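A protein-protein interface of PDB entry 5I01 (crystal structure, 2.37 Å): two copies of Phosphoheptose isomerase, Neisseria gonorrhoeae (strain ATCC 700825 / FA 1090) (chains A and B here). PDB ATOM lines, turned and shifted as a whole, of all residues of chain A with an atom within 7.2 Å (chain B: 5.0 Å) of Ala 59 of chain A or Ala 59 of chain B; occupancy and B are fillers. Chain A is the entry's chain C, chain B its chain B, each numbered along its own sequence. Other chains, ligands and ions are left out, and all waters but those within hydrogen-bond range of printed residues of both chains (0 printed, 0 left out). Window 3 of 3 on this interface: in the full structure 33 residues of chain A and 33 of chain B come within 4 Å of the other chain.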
ATOM      1  N   GLY A  53     -35.839  -7.057 -17.796  1.00  0.00           N
ATOM      2  CA  GLY A  53     -35.700  -6.622 -19.178  1.00  0.00           C
ATOM      3  C   GLY A  53     -35.471  -7.823 -20.072  1.00  0.00           C
ATOM      4  O   GLY A  53     -35.332  -8.932 -19.572  1.00  0.00           O
ATOM      5  N   ASN A  54     -35.411  -7.616 -21.388  1.00  0.00           N
ATOM      6  CA  ASN A  54     -35.165  -8.713 -22.346  1.00  0.00           C
ATOM      7  C   ASN A  54     -33.841  -8.559 -23.116  1.00  0.00           C
ATOM      8  O   ASN A  54     -33.386  -7.434 -23.400  1.00  0.00           O
ATOM      9  CB  ASN A  54     -36.338  -8.825 -23.335  1.00  0.00           C
ATOM     10  CG  ASN A  54     -37.678  -8.973 -22.631  1.00  0.00           C
ATOM     11  OD1 ASN A  54     -38.178 -10.079 -22.457  1.00  0.00           O
ATOM     12  ND2 ASN A  54     -38.248  -7.861 -22.181  1.00  0.00           N
ATOM     13  N   GLY A  55     -33.220  -9.692 -23.442  1.00  0.00           N
ATOM     14  CA  GLY A  55     -32.009  -9.712 -24.269  1.00  0.00           C
ATOM     15  C   GLY A  55     -30.806  -9.118 -23.565  1.00  0.00           C
ATOM     16  O   GLY A  55     -30.433  -9.551 -22.475  1.00  0.00           O
ATOM     17  N   GLY A  56     -30.207  -8.108 -24.190  1.00  0.00           N
ATOM     18  CA  GLY A  56     -29.128  -7.342 -23.573  1.00  0.00           C
ATOM     19  C   GLY A  56     -29.586  -6.606 -22.326  1.00  0.00           C
ATOM     20  O   GLY A  56     -28.809  -6.417 -21.384  1.00  0.00           O
ATOM     21  N   SER A  57     -30.855  -6.203 -22.311  1.00  0.00           N
ATOM     22  CA  SER A  57     -31.436  -5.582 -21.134  1.00  0.00           C
ATOM     23  C   SER A  57     -31.626  -6.578 -19.991  1.00  0.00           C
ATOM     24  O   SER A  57     -31.665  -6.157 -18.842  1.00  0.00           O
ATOM     25  CB  SER A  57     -32.763  -4.910 -21.480  1.00  0.00           C
ATOM     26  OG  SER A  57     -32.624  -4.014 -22.568  1.00  0.00           O
ATOM     27  N   ALA A  58     -31.744  -7.876 -20.298  1.00  0.00           N
ATOM     28  CA  ALA A  58     -31.771  -8.932 -19.261  1.00  0.00           C
ATOM     29  C   ALA A  58     -30.399  -9.110 -18.640  1.00  0.00           C
ATOM     30  O   ALA A  58     -30.285  -9.290 -17.432  1.00  0.00           O
ATOM     31  CB  ALA A  58     -32.275 -10.261 -19.814  1.00  0.00           C
ATOM     32  N   ALA A  59     -29.364  -9.061 -19.478  1.00  0.00           N
ATOM     33  CA  ALA A  59     -27.979  -9.027 -19.009  1.00  0.00           C
ATOM     34  C   ALA A  59     -27.713  -7.832 -18.091  1.00  0.00           C
ATOM     35  O   ALA A  59     -27.046  -7.977 -17.063  1.00  0.00           O
ATOM     36  CB  ALA A  59     -27.009  -9.004 -20.189  1.00  0.00           C
ATOM     37  N   ASP A  60     -28.248  -6.671 -18.464  1.00  0.00           N
ATOM     38  CA  ASP A  60     -28.119  -5.445 -17.665  1.00  0.00           C
ATOM     39  C   ASP A  60     -28.866  -5.529 -16.335  1.00  0.00           C
ATOM     40  O   ASP A  60     -28.478  -4.891 -15.372  1.00  0.00           O
ATOM     41  CB  ASP A  60     -28.579  -4.207 -18.460  1.00  0.00           C
ATOM     42  CG  ASP A  60     -27.701  -3.921 -19.713  1.00  0.00           C
ATOM     43  OD1 ASP A  60     -26.669  -4.626 -19.950  1.00  0.00           O
ATOM     44  OD2 ASP A  60     -28.064  -2.984 -20.476  1.00  0.00           O
ATOM     45  N   ALA A  61     -29.927  -6.316 -16.273  1.00  0.00           N
ATOM     46  CA  ALA A  61     -30.655  -6.509 -15.020  1.00  0.00           C
ATOM     47  C   ALA A  61     -29.848  -7.318 -14.008  1.00  0.00           C
ATOM     48  O   ALA A  61     -29.868  -7.015 -12.805  1.00  0.00           O
ATOM     49  CB  ALA A  61     -31.996  -7.168 -15.277  1.00  0.00           C
ATOM     50  N   GLN A  62     -29.147  -8.346 -14.477  1.00  0.00           N
ATOM     51  CA  GLN A  62     -28.368  -9.181 -13.577  1.00  0.00           C
ATOM     52  C   GLN A  62     -27.014  -8.541 -13.210  1.00  0.00           C
ATOM     53  O   GLN A  62     -26.494  -8.778 -12.122  1.00  0.00           O
ATOM     54  CB  GLN A  62     -28.261 -10.621 -14.112  1.00  0.00           C
ATOM     55  CG  GLN A  62     -27.208 -10.937 -15.164  1.00  0.00           C
ATOM     56  CD  GLN A  62     -27.224 -12.417 -15.557  1.00  0.00           C
ATOM     57  OE1 GLN A  62     -28.298 -12.992 -15.816  1.00  0.00           O
ATOM     58  NE2 GLN A  62     -26.038 -13.042 -15.603  1.00  0.00           N
ATOM     59  N   HIS A  63     -26.474  -7.722 -14.113  1.00  0.00           N
ATOM     60  CA  HIS A  63     -25.260  -6.923 -13.877  1.00  0.00           C
ATOM     61  C   HIS A  63     -25.501  -6.001 -12.687  1.00  0.00           C
ATOM     62  O   HIS A  63     -24.765  -6.037 -11.712  1.00  0.00           O
ATOM     63  CB  HIS A  63     -24.960  -6.120 -15.154  1.00  0.00           C
ATOM     64  CG  HIS A  63     -23.675  -5.353 -15.149  1.00  0.00           C
ATOM     65  ND1 HIS A  63     -22.994  -5.080 -16.315  1.00  0.00           N
ATOM     66  CD2 HIS A  63     -22.962  -4.776 -14.153  1.00  0.00           C
ATOM     67  CE1 HIS A  63     -21.912  -4.375 -16.038  1.00  0.00           C
ATOM     68  NE2 HIS A  63     -21.873  -4.173 -14.735  1.00  0.00           N
ATOM     69  N   PHE A  64     -26.564  -5.207 -12.776  1.00  0.00           N
ATOM     70  CA  PHE A  64     -26.981  -4.287 -11.717  1.00  0.00           C
ATOM     71  C   PHE A  64     -27.225  -5.007 -10.388  1.00  0.00           C
ATOM     72  O   PHE A  64     -26.677  -4.606  -9.365  1.00  0.00           O
ATOM     73  CB  PHE A  64     -28.245  -3.515 -12.147  1.00  0.00           C
ATOM     74  CG  PHE A  64     -28.965  -2.858 -11.013  1.00  0.00           C
ATOM     75  CD1 PHE A  64     -28.453  -1.712 -10.421  1.00  0.00           C
ATOM     76  CD2 PHE A  64     -30.145  -3.404 -10.517  1.00  0.00           C
ATOM     77  CE1 PHE A  64     -29.112  -1.107  -9.352  1.00  0.00           C
ATOM     78  CE2 PHE A  64     -30.809  -2.813  -9.451  1.00  0.00           C
ATOM     79  CZ  PHE A  64     -30.293  -1.664  -8.863  1.00  0.00           C
ATOM     80  N   ALA A  65     -28.030  -6.064 -10.413  1.00  0.00           N
ATOM     81  CA  ALA A  65     -28.315  -6.835  -9.204  1.00  0.00           C
ATOM     82  C   ALA A  65     -27.056  -7.394  -8.557  1.00  0.00           C
ATOM     83  O   ALA A  65     -26.970  -7.453  -7.337  1.00  0.00           O
ATOM     84  CB  ALA A  65     -29.283  -7.966  -9.496  1.00  0.00           C
ATOM     85  N   THR A  85     -34.805 -12.132 -14.125  1.00  0.00           N
ATOM     86  CA  THR A  85     -34.477 -12.633 -15.444  1.00  0.00           C
ATOM     87  C   THR A  85     -33.571 -13.859 -15.351  1.00  0.00           C
ATOM     88  O   THR A  85     -33.059 -14.302 -16.354  1.00  0.00           O
ATOM     89  CB  THR A  85     -33.749 -11.528 -16.235  1.00  0.00           C
ATOM     90  OG1 THR A  85     -32.565 -11.119 -15.529  1.00  0.00           O
ATOM     91  CG2 THR A  85     -34.655 -10.307 -16.424  1.00  0.00           C
ATOM     92  N   ILE A 121     -36.390  -2.390 -17.766  1.00  0.00           N
ATOM     93  CA  ILE A 121     -35.464  -1.978 -18.833  1.00  0.00           C
ATOM     94  C   ILE A 121     -36.025  -2.441 -20.174  1.00  0.00           C
ATOM     95  O   ILE A 121     -36.300  -3.624 -20.357  1.00  0.00           O
ATOM     96  CB  ILE A 121     -34.024  -2.528 -18.636  1.00  0.00           C
ATOM     97  CG1 ILE A 121     -33.504  -2.243 -17.217  1.00  0.00           C
ATOM     98  CG2 ILE A 121     -33.049  -1.898 -19.640  1.00  0.00           C
ATOM     99  CD1 ILE A 121     -32.276  -3.044 -16.832  1.00  0.00           C
ATOM    100  N   ILE A 181     -26.102   0.755 -19.270  1.00  0.00           N
ATOM    101  CA  ILE A 181     -25.039   0.272 -18.368  1.00  0.00           C
ATOM    102  C   ILE A 181     -24.304   1.409 -17.695  1.00  0.00           C
ATOM    103  O   ILE A 181     -23.972   1.284 -16.525  1.00  0.00           O
ATOM    104  CB  ILE A 181     -23.990  -0.669 -19.019  1.00  0.00           C
ATOM    105  CG1 ILE A 181     -23.384  -0.008 -20.254  1.00  0.00           C
ATOM    106  CG2 ILE A 181     -24.614  -2.015 -19.360  1.00  0.00           C
ATOM    107  CD1 ILE A 181     -22.374  -0.826 -20.998  1.00  0.00           C
ATOM    108  N   ILE A 184     -26.581   2.735 -15.033  1.00  0.00           N
ATOM    109  CA  ILE A 184     -26.512   1.766 -13.934  1.00  0.00           C
ATOM    110  C   ILE A 184     -25.262   1.917 -13.075  1.00  0.00           C
ATOM    111  O   ILE A 184     -25.353   1.812 -11.858  1.00  0.00           O
ATOM    112  CB  ILE A 184     -26.645   0.326 -14.467  1.00  0.00           C
ATOM    113  CG1 ILE A 184     -28.098   0.092 -14.875  1.00  0.00           C
ATOM    114  CG2 ILE A 184     -26.224  -0.713 -13.431  1.00  0.00           C
ATOM    115  CD1 ILE A 184     -28.305  -1.118 -15.750  1.00  0.00           C
ATOM    116  N   GLY B  55     -18.830 -11.585 -13.141  1.00  0.00           N
ATOM    117  CA  GLY B  55     -19.556 -10.366 -12.754  1.00  0.00           C
ATOM    118  C   GLY B  55     -20.274  -9.728 -13.928  1.00  0.00           C
ATOM    119  O   GLY B  55     -21.053 -10.392 -14.626  1.00  0.00           O
ATOM    120  N   GLY B  56     -20.004  -8.441 -14.152  1.00  0.00           N
ATOM    121  CA  GLY B  56     -20.436  -7.758 -15.371  1.00  0.00           C
ATOM    122  C   GLY B  56     -19.942  -8.417 -16.658  1.00  0.00           C
ATOM    123  O   GLY B  56     -20.639  -8.407 -17.666  1.00  0.00           O
ATOM    124  N   SER B  57     -18.748  -9.002 -16.625  1.00  0.00           N
ATOM    125  CA  SER B  57     -18.212  -9.728 -17.778  1.00  0.00           C
ATOM    126  C   SER B  57     -18.986 -11.028 -18.086  1.00  0.00           C
ATOM    127  O   SER B  57     -18.987 -11.499 -19.227  1.00  0.00           O
ATOM    128  CB  SER B  57     -16.736 -10.020 -17.562  1.00  0.00           C
ATOM    129  OG  SER B  57     -16.023  -8.829 -17.232  1.00  0.00           O
ATOM    130  N   ALA B  58     -19.646 -11.593 -17.070  1.00  0.00           N
ATOM    131  CA  ALA B  58     -20.513 -12.748 -17.255  1.00  0.00           C
ATOM    132  C   ALA B  58     -21.780 -12.301 -17.948  1.00  0.00           C
ATOM    133  O   ALA B  58     -22.292 -13.004 -18.797  1.00  0.00           O
ATOM    134  CB  ALA B  58     -20.842 -13.413 -15.923  1.00  0.00           C
ATOM    135  N   ALA B  59     -22.284 -11.127 -17.574  1.00  0.00           N
ATOM    136  CA  ALA B  59     -23.407 -10.510 -18.278  1.00  0.00           C
ATOM    137  C   ALA B  59     -23.035 -10.183 -19.729  1.00  0.00           C
ATOM    138  O   ALA B  59     -23.836 -10.406 -20.631  1.00  0.00           O
ATOM    139  CB  ALA B  59     -23.884  -9.261 -17.549  1.00  0.00           C
ATOM    140  N   ASP B  60     -21.818  -9.686 -19.946  1.00  0.00           N
ATOM    141  CA  ASP B  60     -21.306  -9.421 -21.308  1.00  0.00           C
ATOM    142  C   ASP B  60     -21.216 -10.682 -22.168  1.00  0.00           C
ATOM    143  O   ASP B  60     -21.623 -10.668 -23.312  1.00  0.00           O
ATOM    144  CB  ASP B  60     -19.932  -8.741 -21.264  1.00  0.00           C
ATOM    145  CG  ASP B  60     -19.946  -7.439 -20.472  1.00  0.00           C
ATOM    146  OD1 ASP B  60     -21.048  -6.875 -20.249  1.00  0.00           O
ATOM    147  OD2 ASP B  60     -18.851  -6.993 -20.053  1.00  0.00           O
ATOM    148  N   ALA B  61     -20.715 -11.766 -21.603  1.00  0.00           N
ATOM    149  CA  ALA B  61     -20.598 -13.017 -22.338  1.00  0.00           C
ATOM    150  C   ALA B  61     -21.944 -13.507 -22.883  1.00  0.00           C
ATOM    151  O   ALA B  61     -22.023 -13.922 -24.045  1.00  0.00           O
ATOM    152  CB  ALA B  61     -19.956 -14.088 -21.469  1.00  0.00           C
ATOM    153  N   GLN B  62     -22.999 -13.448 -22.071  1.00  0.00           N
ATOM    154  CA  GLN B  62     -24.314 -13.937 -22.528  1.00  0.00           C
ATOM    155  C   GLN B  62     -25.080 -12.950 -23.409  1.00  0.00           C
ATOM    156  O   GLN B  62     -25.896 -13.361 -24.230  1.00  0.00           O
ATOM    157  CB  GLN B  62     -25.165 -14.422 -21.359  1.00  0.00           C
ATOM    158  CG  GLN B  62     -25.798 -13.358 -20.481  1.00  0.00           C
ATOM    159  CD  GLN B  62     -26.617 -13.982 -19.356  1.00  0.00           C
ATOM    160  OE1 GLN B  62     -26.106 -14.815 -18.586  1.00  0.00           O
ATOM    161  NE2 GLN B  62     -27.893 -13.591 -19.256  1.00  0.00           N
ATOM    162  N   HIS B  63     -24.823 -11.656 -23.220  1.00  0.00           N
ATOM    163  CA  HIS B  63     -25.291 -10.602 -24.125  1.00  0.00           C
ATOM    164  C   HIS B  63     -24.775 -10.904 -25.543  1.00  0.00           C
ATOM    165  O   HIS B  63     -25.552 -10.945 -26.489  1.00  0.00           O
ATOM    166  CB  HIS B  63     -24.765  -9.250 -23.626  1.00  0.00           C
ATOM    167  CG  HIS B  63     -25.288  -8.054 -24.363  1.00  0.00           C
ATOM    168  ND1 HIS B  63     -25.567  -6.875 -23.712  1.00  0.00           N
ATOM    169  CD2 HIS B  63     -25.545  -7.829 -25.674  1.00  0.00           C
ATOM    170  CE1 HIS B  63     -25.984  -5.977 -24.584  1.00  0.00           C
ATOM    171  NE2 HIS B  63     -25.980  -6.530 -25.782  1.00  0.00           N
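OE1 of Gln 62 of chain B sits at hydrogen-bond distance from NE2 of Gln 62 of chain A (3.5 Å).
His 63 of chain B touches Gly 56 of chain A. Ala 59 of chain A touches Ala 59 of chain B (O to CB, 3.4 Å). His 63 of chain A touches Gly 56 of chain B (CE1 to CA, 3.8 Å).
Of the printed residues of chain B, Ala 59 of chain A touches Ala 59 (3.4 Å). Of the printed residues of chain B, Gln 62 of chain A touches Gln 62 (3.5 Å). Of the printed residues of chain A, Gly 56 of chain B touches His 63 (3.8 Å). Of the printed residues of chain A, Ala 59 of chain B touches Ala 59 (3.4 Å). The nearest residue of chain B that does not touch Ala 59 of chain A is His 63 of chain B (4.1 Å). The nearest residue of chain A that does not touch Ala 59 of chain B is His 63 of chain A (4.1 Å). The nearest printed residue of chain B that does not touch Gln 62 of chain A is Ala 59 of chain B (4.4 Å).
Of the 17 printed residues of chain A, 4 touch a printed residue of chain B. Of the 9 printed residues of chain B, 4 touch a printed residue of chain A. Among the printed residues, 4 pairs touch across the chains. Among the printed residues, no Asp or Glu carboxylate lies within 4 Å of a Lys or Arg side-chain nitrogen of the other chain.
Gly 56 of chain A touches His 63 of chain B, and with the chains exchanged His 63 of chain A touches Gly 56 of chain B. Ala 59 of chain B touches its own counterpart, Ala 59 of chain A. Gln 62 of chain A touches its own counterpart, Gln 62 of chain B. 9 positions are printed for both chains. Of the 4 pairs that touch across the chains among the printed residues, 4 have their exchanged pair printed and touching as well.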
